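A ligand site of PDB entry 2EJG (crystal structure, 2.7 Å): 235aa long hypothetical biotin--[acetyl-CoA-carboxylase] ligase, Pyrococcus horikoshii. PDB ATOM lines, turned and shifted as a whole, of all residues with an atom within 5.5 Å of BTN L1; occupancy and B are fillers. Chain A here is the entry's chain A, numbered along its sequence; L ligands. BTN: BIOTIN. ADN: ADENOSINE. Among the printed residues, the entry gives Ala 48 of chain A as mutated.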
ATOM      1  N   THR A  20      -7.741 -16.598  26.994  1.00  0.00           N
ATOM      2  CA  THR A  20      -8.396 -16.708  25.689  1.00  0.00           C
ATOM      3  C   THR A  20      -8.011 -18.030  25.047  1.00  0.00           C
ATOM      4  O   THR A  20      -8.865 -18.779  24.591  1.00  0.00           O
ATOM      5  CB  THR A  20      -8.018 -15.528  24.739  1.00  0.00           C
ATOM      6  OG1 THR A  20      -6.596 -15.338  24.726  1.00  0.00           O
ATOM      7  CG2 THR A  20      -8.705 -14.221  25.196  1.00  0.00           C
ATOM      8  N   SER A  21      -6.712 -18.317  25.038  1.00  0.00           N
ATOM      9  CA  SER A  21      -6.210 -19.553  24.459  1.00  0.00           C
ATOM     10  C   SER A  21      -4.783 -19.833  24.911  1.00  0.00           C
ATOM     11  O   SER A  21      -3.932 -18.958  24.874  1.00  0.00           O
ATOM     12  CB  SER A  21      -6.247 -19.474  22.922  1.00  0.00           C
ATOM     13  OG  SER A  21      -5.639 -20.606  22.312  1.00  0.00           O
ATOM     14  N   THR A  22      -4.525 -21.068  25.333  1.00  0.00           N
ATOM     15  CA  THR A  22      -3.185 -21.445  25.754  1.00  0.00           C
ATOM     16  C   THR A  22      -2.283 -21.464  24.531  1.00  0.00           C
ATOM     17  O   THR A  22      -1.134 -21.040  24.596  1.00  0.00           O
ATOM     18  CB  THR A  22      -3.132 -22.854  26.390  1.00  0.00           C
ATOM     19  OG1 THR A  22      -3.849 -23.786  25.570  1.00  0.00           O
ATOM     20  CG2 THR A  22      -3.719 -22.826  27.804  1.00  0.00           C
ATOM     21  N   ASN A  23      -2.817 -21.947  23.409  1.00  0.00           N
ATOM     22  CA  ASN A  23      -2.027 -22.014  22.189  1.00  0.00           C
ATOM     23  C   ASN A  23      -1.553 -20.635  21.737  1.00  0.00           C
ATOM     24  O   ASN A  23      -0.376 -20.459  21.393  1.00  0.00           O
ATOM     25  CB  ASN A  23      -2.807 -22.690  21.051  1.00  0.00           C
ATOM     26  CG  ASN A  23      -2.406 -24.152  20.845  1.00  0.00           C
ATOM     27  OD1 ASN A  23      -1.788 -24.767  21.717  1.00  0.00           O
ATOM     28  ND2 ASN A  23      -2.745 -24.693  19.684  1.00  0.00           N
ATOM     29  N   GLN A  42     -10.516 -21.779  29.095  1.00  0.00           N
ATOM     30  CA  GLN A  42     -10.157 -20.912  27.974  1.00  0.00           C
ATOM     31  C   GLN A  42     -11.467 -20.307  27.471  1.00  0.00           C
ATOM     32  O   GLN A  42     -12.522 -20.945  27.561  1.00  0.00           O
ATOM     33  CB  GLN A  42      -9.538 -21.687  26.816  1.00  0.00           C
ATOM     34  CG  GLN A  42      -8.347 -22.597  27.078  1.00  0.00           C
ATOM     35  CD  GLN A  42      -7.746 -23.063  25.739  1.00  0.00           C
ATOM     36  OE1 GLN A  42      -6.811 -22.470  25.232  1.00  0.00           O
ATOM     37  NE2 GLN A  42      -8.330 -24.099  25.153  1.00  0.00           N
ATOM     38  N   MET A  44     -11.443 -18.211  24.381  1.00  0.00           N
ATOM     39  CA  MET A  44     -11.322 -18.186  22.943  1.00  0.00           C
ATOM     40  C   MET A  44     -10.722 -19.512  22.457  1.00  0.00           C
ATOM     41  O   MET A  44      -9.890 -19.513  21.541  1.00  0.00           O
ATOM     42  CB  MET A  44     -10.438 -17.033  22.491  1.00  0.00           C
ATOM     43  CG  MET A  44     -10.938 -15.661  22.918  1.00  0.00           C
ATOM     44  SD  MET A  44     -12.659 -15.370  22.501  1.00  0.00           S
ATOM     45  CE  MET A  44     -13.164 -14.261  23.860  1.00  0.00           C
ATOM     46  N   GLY A  45     -11.139 -20.614  23.066  1.00  0.00           N
ATOM     47  CA  GLY A  45     -10.633 -21.912  22.686  1.00  0.00           C
ATOM     48  C   GLY A  45     -10.601 -22.129  21.191  1.00  0.00           C
ATOM     49  O   GLY A  45     -11.511 -21.718  20.473  1.00  0.00           O
ATOM     50  N   HIS A  46      -9.553 -22.784  20.707  1.00  0.00           N
ATOM     51  CA  HIS A  46      -9.394 -23.038  19.267  1.00  0.00           C
ATOM     52  C   HIS A  46      -9.412 -24.522  18.877  1.00  0.00           C
ATOM     53  O   HIS A  46      -9.101 -25.395  19.669  1.00  0.00           O
ATOM     54  CB  HIS A  46      -8.095 -22.402  18.773  1.00  0.00           C
ATOM     55  CG  HIS A  46      -8.114 -20.905  18.765  1.00  0.00           C
ATOM     56  ND1 HIS A  46      -6.981 -20.142  18.887  1.00  0.00           N
ATOM     57  CD2 HIS A  46      -9.143 -20.034  18.611  1.00  0.00           C
ATOM     58  CE1 HIS A  46      -7.306 -18.862  18.819  1.00  0.00           C
ATOM     59  NE2 HIS A  46      -8.606 -18.770  18.654  1.00  0.00           N
ATOM     60  N   GLY A  47      -9.790 -24.771  17.631  1.00  0.00           N
ATOM     61  CA  GLY A  47      -9.837 -26.132  17.115  1.00  0.00           C
ATOM     62  C   GLY A  47      -9.200 -26.194  15.745  1.00  0.00           C
ATOM     63  O   GLY A  47      -8.953 -25.165  15.097  1.00  0.00           O
ATOM     64  N   ALA A  48      -8.930 -27.414  15.280  1.00  0.00           N
ATOM     65  CA  ALA A  48      -8.305 -27.611  13.985  1.00  0.00           C
ATOM     66  C   ALA A  48      -9.164 -27.031  12.873  1.00  0.00           C
ATOM     67  O   ALA A  48     -10.378 -26.992  12.980  1.00  0.00           O
ATOM     68  CB  ALA A  48      -8.064 -29.095  13.751  1.00  0.00           C
ATOM     69  N   ARG A  51     -12.006 -24.156  13.383  1.00  0.00           N
ATOM     70  CA  ARG A  51     -13.183 -24.470  14.190  1.00  0.00           C
ATOM     71  C   ARG A  51     -12.973 -23.930  15.603  1.00  0.00           C
ATOM     72  O   ARG A  51     -11.913 -23.391  15.924  1.00  0.00           O
ATOM     73  CB  ARG A  51     -13.435 -25.979  14.276  1.00  0.00           C
ATOM     74  CG  ARG A  51     -13.828 -26.580  12.936  1.00  0.00           C
ATOM     75  CD  ARG A  51     -13.306 -28.007  12.839  1.00  0.00           C
ATOM     76  NE  ARG A  51     -13.663 -28.654  11.584  1.00  0.00           N
ATOM     77  CZ  ARG A  51     -12.844 -29.512  11.004  1.00  0.00           C
ATOM     78  NH1 ARG A  51     -11.674 -29.749  11.577  1.00  0.00           N
ATOM     79  NH2 ARG A  51     -13.190 -30.174   9.916  1.00  0.00           N
ATOM     80  N   TRP A  53     -13.325 -24.490  20.043  1.00  0.00           N
ATOM     81  CA  TRP A  53     -13.197 -25.515  21.060  1.00  0.00           C
ATOM     82  C   TRP A  53     -13.684 -25.111  22.457  1.00  0.00           C
ATOM     83  O   TRP A  53     -13.185 -24.168  23.054  1.00  0.00           O
ATOM     84  CB  TRP A  53     -11.741 -25.990  21.153  1.00  0.00           C
ATOM     85  CG  TRP A  53     -11.554 -27.094  22.142  1.00  0.00           C
ATOM     86  CD1 TRP A  53     -11.288 -26.954  23.471  1.00  0.00           C
ATOM     87  CD2 TRP A  53     -11.685 -28.497  21.903  1.00  0.00           C
ATOM     88  NE1 TRP A  53     -11.247 -28.188  24.080  1.00  0.00           N
ATOM     89  CE2 TRP A  53     -11.494 -29.153  23.140  1.00  0.00           C
ATOM     90  CE3 TRP A  53     -11.955 -29.272  20.769  1.00  0.00           C
ATOM     91  CZ2 TRP A  53     -11.559 -30.548  23.270  1.00  0.00           C
ATOM     92  CZ3 TRP A  53     -12.020 -30.667  20.899  1.00  0.00           C
ATOM     93  CH2 TRP A  53     -11.825 -31.284  22.149  1.00  0.00           C
ATOM     94  N   SER A  55     -13.859 -25.016  26.209  1.00  0.00           N
ATOM     95  CA  SER A  55     -12.915 -25.254  27.288  1.00  0.00           C
ATOM     96  C   SER A  55     -13.504 -24.872  28.631  1.00  0.00           C
ATOM     97  O   SER A  55     -13.030 -23.948  29.290  1.00  0.00           O
ATOM     98  CB  SER A  55     -11.657 -24.439  27.057  1.00  0.00           C
ATOM     99  OG  SER A  55     -11.336 -24.398  25.692  1.00  0.00           O
ATOM    100  N   LEU A  60      -8.853 -30.484  31.034  1.00  0.00           N
ATOM    101  CA  LEU A  60      -7.435 -30.181  30.905  1.00  0.00           C
ATOM    102  C   LEU A  60      -7.144 -29.534  29.545  1.00  0.00           C
ATOM    103  O   LEU A  60      -7.273 -30.176  28.490  1.00  0.00           O
ATOM    104  CB  LEU A  60      -6.640 -31.482  31.085  1.00  0.00           C
ATOM    105  CG  LEU A  60      -5.124 -31.421  31.152  1.00  0.00           C
ATOM    106  CD1 LEU A  60      -4.663 -30.446  32.222  1.00  0.00           C
ATOM    107  CD2 LEU A  60      -4.620 -32.829  31.441  1.00  0.00           C
ATOM    108  N   TRP A  61      -6.788 -28.248  29.577  1.00  0.00           N
ATOM    109  CA  TRP A  61      -6.489 -27.467  28.366  1.00  0.00           C
ATOM    110  C   TRP A  61      -5.047 -26.996  28.467  1.00  0.00           C
ATOM    111  O   TRP A  61      -4.749 -26.085  29.232  1.00  0.00           O
ATOM    112  CB  TRP A  61      -7.417 -26.244  28.256  1.00  0.00           C
ATOM    113  CG  TRP A  61      -8.773 -26.503  28.828  1.00  0.00           C
ATOM    114  CD1 TRP A  61      -9.336 -25.903  29.940  1.00  0.00           C
ATOM    115  CD2 TRP A  61      -9.708 -27.487  28.389  1.00  0.00           C
ATOM    116  NE1 TRP A  61     -10.557 -26.477  30.215  1.00  0.00           N
ATOM    117  CE2 TRP A  61     -10.810 -27.456  29.277  1.00  0.00           C
ATOM    118  CE3 TRP A  61      -9.722 -28.413  27.333  1.00  0.00           C
ATOM    119  CZ2 TRP A  61     -11.917 -28.303  29.141  1.00  0.00           C
ATOM    120  CZ3 TRP A  61     -10.829 -29.260  27.196  1.00  0.00           C
ATOM    121  CH2 TRP A  61     -11.902 -29.194  28.093  1.00  0.00           C
ATOM    122  N   LEU A  62      -4.171 -27.617  27.681  1.00  0.00           N
ATOM    123  CA  LEU A  62      -2.748 -27.263  27.722  1.00  0.00           C
ATOM    124  C   LEU A  62      -2.039 -27.135  26.376  1.00  0.00           C
ATOM    125  O   LEU A  62      -2.519 -27.630  25.358  1.00  0.00           O
ATOM    126  CB  LEU A  62      -2.008 -28.264  28.611  1.00  0.00           C
ATOM    127  CG  LEU A  62      -2.107 -29.764  28.288  1.00  0.00           C
ATOM    128  CD1 LEU A  62      -1.333 -30.098  27.026  1.00  0.00           C
ATOM    129  CD2 LEU A  62      -1.557 -30.552  29.465  1.00  0.00           C
ATOM    130  N   SER A  63      -0.902 -26.457  26.415  1.00  0.00           N
ATOM    131  CA  SER A  63      -0.044 -26.210  25.260  1.00  0.00           C
ATOM    132  C   SER A  63       1.409 -26.490  25.623  1.00  0.00           C
ATOM    133  O   SER A  63       1.894 -26.079  26.685  1.00  0.00           O
ATOM    134  CB  SER A  63      -0.175 -24.763  24.807  1.00  0.00           C
ATOM    135  OG  SER A  63      -1.512 -24.462  24.481  1.00  0.00           O
ATOM    136  N   ASN A 103      -6.401 -36.218  14.576  1.00  0.00           N
ATOM    137  CA  ASN A 103      -6.184 -35.400  15.791  1.00  0.00           C
ATOM    138  C   ASN A 103      -7.261 -35.597  16.894  1.00  0.00           C
ATOM    139  O   ASN A 103      -7.280 -34.855  17.872  1.00  0.00           O
ATOM    140  CB  ASN A 103      -6.103 -33.925  15.367  1.00  0.00           C
ATOM    141  CG  ASN A 103      -7.453 -33.435  14.925  1.00  0.00           C
ATOM    142  OD1 ASN A 103      -8.155 -34.070  14.139  1.00  0.00           O
ATOM    143  ND2 ASN A 103      -7.883 -32.303  15.518  1.00  0.00           N
ATOM    144  N   ASP A 104      -8.170 -36.555  16.755  1.00  0.00           N
ATOM    145  CA  ASP A 104      -9.178 -36.755  17.781  1.00  0.00           C
ATOM    146  C   ASP A 104      -9.083 -38.136  18.421  1.00  0.00           C
ATOM    147  O   ASP A 104      -8.828 -39.125  17.743  1.00  0.00           O
ATOM    148  CB  ASP A 104     -10.592 -36.609  17.186  1.00  0.00           C
ATOM    149  CG  ASP A 104     -10.745 -35.389  16.305  1.00  0.00           C
ATOM    150  OD1 ASP A 104     -10.451 -34.263  16.767  1.00  0.00           O
ATOM    151  OD2 ASP A 104     -11.167 -35.560  15.133  1.00  0.00           O
ATOM    152  N   LYS A 111     -16.283 -38.095  21.113  1.00  0.00           N
ATOM    153  CA  LYS A 111     -15.067 -37.306  21.262  1.00  0.00           C
ATOM    154  C   LYS A 111     -14.734 -36.941  22.691  1.00  0.00           C
ATOM    155  O   LYS A 111     -15.555 -36.366  23.386  1.00  0.00           O
ATOM    156  CB  LYS A 111     -15.169 -36.017  20.431  1.00  0.00           C
ATOM    157  CG  LYS A 111     -13.822 -35.333  20.248  1.00  0.00           C
ATOM    158  CD  LYS A 111     -13.862 -34.256  19.167  1.00  0.00           C
ATOM    159  CE  LYS A 111     -12.493 -33.597  19.050  1.00  0.00           C
ATOM    160  NZ  LYS A 111     -12.411 -32.620  17.943  1.00  0.00           N
ATOM    161  N   ALA A 113     -11.268 -35.834  23.319  1.00  0.00           N
ATOM    162  CA  ALA A 113     -10.086 -34.985  23.197  1.00  0.00           C
ATOM    163  C   ALA A 113      -9.740 -34.675  21.748  1.00  0.00           C
ATOM    164  O   ALA A 113     -10.193 -35.352  20.816  1.00  0.00           O
ATOM    165  CB  ALA A 113      -8.895 -35.644  23.886  1.00  0.00           C
ATOM    166  N   GLY A 114      -8.929 -33.635  21.550  1.00  0.00           N
ATOM    167  CA  GLY A 114      -8.514 -33.248  20.217  1.00  0.00           C
ATOM    168  C   GLY A 114      -7.151 -32.584  20.247  1.00  0.00           C
ATOM    169  O   GLY A 114      -6.779 -31.977  21.249  1.00  0.00           O
ATOM    170  N   VAL A 115      -6.388 -32.699  19.171  1.00  0.00           N
ATOM    171  CA  VAL A 115      -5.076 -32.067  19.130  1.00  0.00           C
ATOM    172  C   VAL A 115      -5.046 -30.981  18.067  1.00  0.00           C
ATOM    173  O   VAL A 115      -5.770 -31.049  17.074  1.00  0.00           O
ATOM    174  CB  VAL A 115      -3.926 -33.089  18.865  1.00  0.00           C
ATOM    175  CG1 VAL A 115      -2.573 -32.437  19.183  1.00  0.00           C
ATOM    176  CG2 VAL A 115      -4.110 -34.320  19.700  1.00  0.00           C
ATOM    177  N   LEU A 116      -4.214 -29.976  18.290  1.00  0.00           N
ATOM    178  CA  LEU A 116      -4.068 -28.862  17.379  1.00  0.00           C
ATOM    179  C   LEU A 116      -2.609 -28.408  17.414  1.00  0.00           C
ATOM    180  O   LEU A 116      -2.131 -27.942  18.450  1.00  0.00           O
ATOM    181  CB  LEU A 116      -4.973 -27.706  17.815  1.00  0.00           C
ATOM    182  CG  LEU A 116      -4.673 -26.306  17.246  1.00  0.00           C
ATOM    183  CD1 LEU A 116      -4.890 -26.280  15.738  1.00  0.00           C
ATOM    184  CD2 LEU A 116      -5.555 -25.286  17.938  1.00  0.00           C
ATOM    185  N   GLY A 127      -0.965 -28.314  21.076  1.00  0.00           N
ATOM    186  CA  GLY A 127      -2.100 -28.034  21.944  1.00  0.00           C
ATOM    187  C   GLY A 127      -2.966 -29.266  22.091  1.00  0.00           C
ATOM    188  O   GLY A 127      -3.264 -29.953  21.108  1.00  0.00           O
ATOM    189  N   ILE A 128      -3.367 -29.563  23.319  1.00  0.00           N
ATOM    190  CA  ILE A 128      -4.192 -30.724  23.565  1.00  0.00           C
ATOM    191  C   ILE A 128      -5.343 -30.378  24.507  1.00  0.00           C
ATOM    192  O   ILE A 128      -5.114 -29.791  25.561  1.00  0.00           O
ATOM    193  CB  ILE A 128      -3.378 -31.867  24.233  1.00  0.00           C
ATOM    194  CG1 ILE A 128      -2.134 -32.188  23.395  1.00  0.00           C
ATOM    195  CG2 ILE A 128      -4.233 -33.098  24.372  1.00  0.00           C
ATOM    196  CD1 ILE A 128      -1.186 -33.158  24.076  1.00  0.00           C
ATOM    197  N   GLY A 129      -6.560 -30.711  24.101  1.00  0.00           N
ATOM    198  CA  GLY A 129      -7.742 -30.478  24.914  1.00  0.00           C
ATOM    199  C   GLY A 129      -8.371 -31.825  25.230  1.00  0.00           C
ATOM    200  O   GLY A 129      -8.781 -32.536  24.319  1.00  0.00           O
HETATM  201  C11 BTN L   1      -9.710 -30.307  17.654  1.00  0.00           C
HETATM  202  O11 BTN L   1     -10.134 -31.431  17.958  1.00  0.00           O
HETATM  203  O12 BTN L   1     -10.266 -29.617  16.747  1.00  0.00           O
HETATM  204  C10 BTN L   1      -8.512 -29.724  18.343  1.00  0.00           C
HETATM  205  C9  BTN L   1      -8.806 -29.157  19.698  1.00  0.00           C
HETATM  206  C8  BTN L   1      -7.590 -28.668  20.448  1.00  0.00           C
HETATM  207  C7  BTN L   1      -7.981 -28.110  21.810  1.00  0.00           C
HETATM  208  C2  BTN L   1      -6.834 -27.580  22.681  1.00  0.00           C
HETATM  209  S1  BTN L   1      -7.345 -26.933  24.286  1.00  0.00           S
HETATM  210  C6  BTN L   1      -5.607 -26.528  24.603  1.00  0.00           C
HETATM  211  C5  BTN L   1      -5.226 -25.799  23.289  1.00  0.00           C
HETATM  212  N1  BTN L   1      -5.602 -24.385  23.269  1.00  0.00           N
HETATM  213  C3  BTN L   1      -6.423 -24.121  22.239  1.00  0.00           C
HETATM  214  O3  BTN L   1      -6.912 -22.976  21.980  1.00  0.00           O
HETATM  215  N2  BTN L   1      -6.682 -25.275  21.506  1.00  0.00           N
HETATM  216  C4  BTN L   1      -5.960 -26.419  22.074  1.00  0.00           C
HETATM  217  O5' ADN L   2     -12.807 -30.743  16.130  1.00  0.00           O
HETATM  218  C5' ADN L   2     -13.929 -29.865  15.992  1.00  0.00           C
HETATM  219  C4' ADN L   2     -15.188 -30.525  16.567  1.00  0.00           C
HETATM  220  O4' ADN L   2     -15.007 -30.799  17.980  1.00  0.00           O
HETATM  221  C3' ADN L   2     -16.418 -29.596  16.428  1.00  0.00           C
HETATM  222  O3' ADN L   2     -17.270 -30.009  15.341  1.00  0.00           O
HETATM  223  C2' ADN L   2     -17.113 -29.615  17.814  1.00  0.00           C
HETATM  224  O2' ADN L   2     -18.485 -30.034  17.761  1.00  0.00           O
HETATM  225  C1' ADN L   2     -16.255 -30.548  18.686  1.00  0.00           C
HETATM  226  N9  ADN L   2     -15.940 -29.935  20.012  1.00  0.00           N
HETATM  227  C8  ADN L   2     -15.756 -28.605  20.306  1.00  0.00           C
HETATM  228  N7  ADN L   2     -15.464 -28.507  21.717  1.00  0.00           N
HETATM  229  C5  ADN L   2     -15.479 -29.732  22.244  1.00  0.00           C
HETATM  230  C6  ADN L   2     -15.275 -30.284  23.543  1.00  0.00           C
HETATM  231  N6  ADN L   2     -14.978 -29.467  24.610  1.00  0.00           N
HETATM  232  N1  ADN L   2     -15.362 -31.640  23.711  1.00  0.00           N
HETATM  233  C2  ADN L   2     -15.642 -32.490  22.690  1.00  0.00           C
HETATM  234  N3  ADN L   2     -15.853 -32.022  21.442  1.00  0.00           N
HETATM  235  C4  ADN L   2     -15.783 -30.664  21.174  1.00  0.00           C
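N of Asn 23 sits close to OG of Ser 21 (3.3 Å).
The backbone NH (N) of Thr 22 sits at hydrogen-bond distance from the side-chain amide oxygen (OE1) of Gln 42.
The side-chain hydroxyl of Thr 22 is in hydrogen-bond range of the side-chain hydroxyl of Ser 63, at 2.7 Å.
The backbone carbonyl oxygen of Ala 48 lies close to the guanidinium group of Arg 51.
The backbone carbonyl oxygen (O) of Gly 129 is in hydrogen-bond range of the backbone NH (N) of Gly 114 (3.0 Å).
N of Trp 53 lies within hydrogen-bond range of O of Gly 45, at 3.3 Å.
The backbone NH (N) of Ile 128 lies within hydrogen-bond range of the backbone carbonyl oxygen (O) of Leu 62 (2.9 Å).
The backbone carbonyl oxygen (O) of Leu 116 is in hydrogen-bond range of the backbone NH (N) of Gly 127 (2.9 Å).
Merely in contact with BTN L1: Asn 23 (3.7 Å), Gly 45 (3.9 Å), Gly 47 (3.5 Å), Trp 53 (3.3 Å), Trp 61 (3.9 Å), Leu 62 (3.4 Å), Gly 114 (3.3 Å), Val 115 (3.3 Å), Leu 116 (3.7 Å), Ile 128 (3.4 Å) and Gly 129 (3.4 Å).
Hydrophobic or aromatic side chains that line BTN L1: His 46, Ala 48, Trp 53 and Leu 116.
Within 4 Å of BTN L1: Ser 21, Thr 22, Asn 23, Gln 42, Gly 45, His 46, Gly 47, Ala 48, Trp 53, Trp 61, Leu 62, Asn 103, Asp 104, Lys 111, Gly 114, Val 115, Leu 116, Ile 128 and Gly 129.
The nearest printed residue that does not touch BTN L1 is Gly 127 (4.1 Å).
An oxygen (O5') of ADN L2 lies within hydrogen-bond range of an oxygen (O12) of BTN L1.
NZ of Lys 111 is in salt-bridge range of O11 of BTN L1 (2.6 Å).
An oxygen (O3) of BTN L1 sits at hydrogen-bond distance from the side-chain hydroxyl (OG) of Ser 21 (2.7 Å).
N of His 46 is in hydrogen-bond range of O3 of BTN L1, at 2.9 Å.
O of His 46 is in hydrogen-bond range of N2 of BTN L1.
N1 of BTN L1 lies within hydrogen-bond range of OG1 of Thr 22 (3.0 Å).
N of Ala 48 lies within hydrogen-bond range of O12 of BTN L1.
OE1 of Gln 42 is in hydrogen-bond range of N1 of BTN L1.
OD1 of Asp 104 sits close to O11 of BTN L1.
The side-chain amide nitrogen of Asn 103 lies within hydrogen-bond range of an oxygen (O11) of BTN L1 (3.4 Å).
NZ of Lys 111 lies within hydrogen-bond range of O5' of ADN L2, at 2.6 Å.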
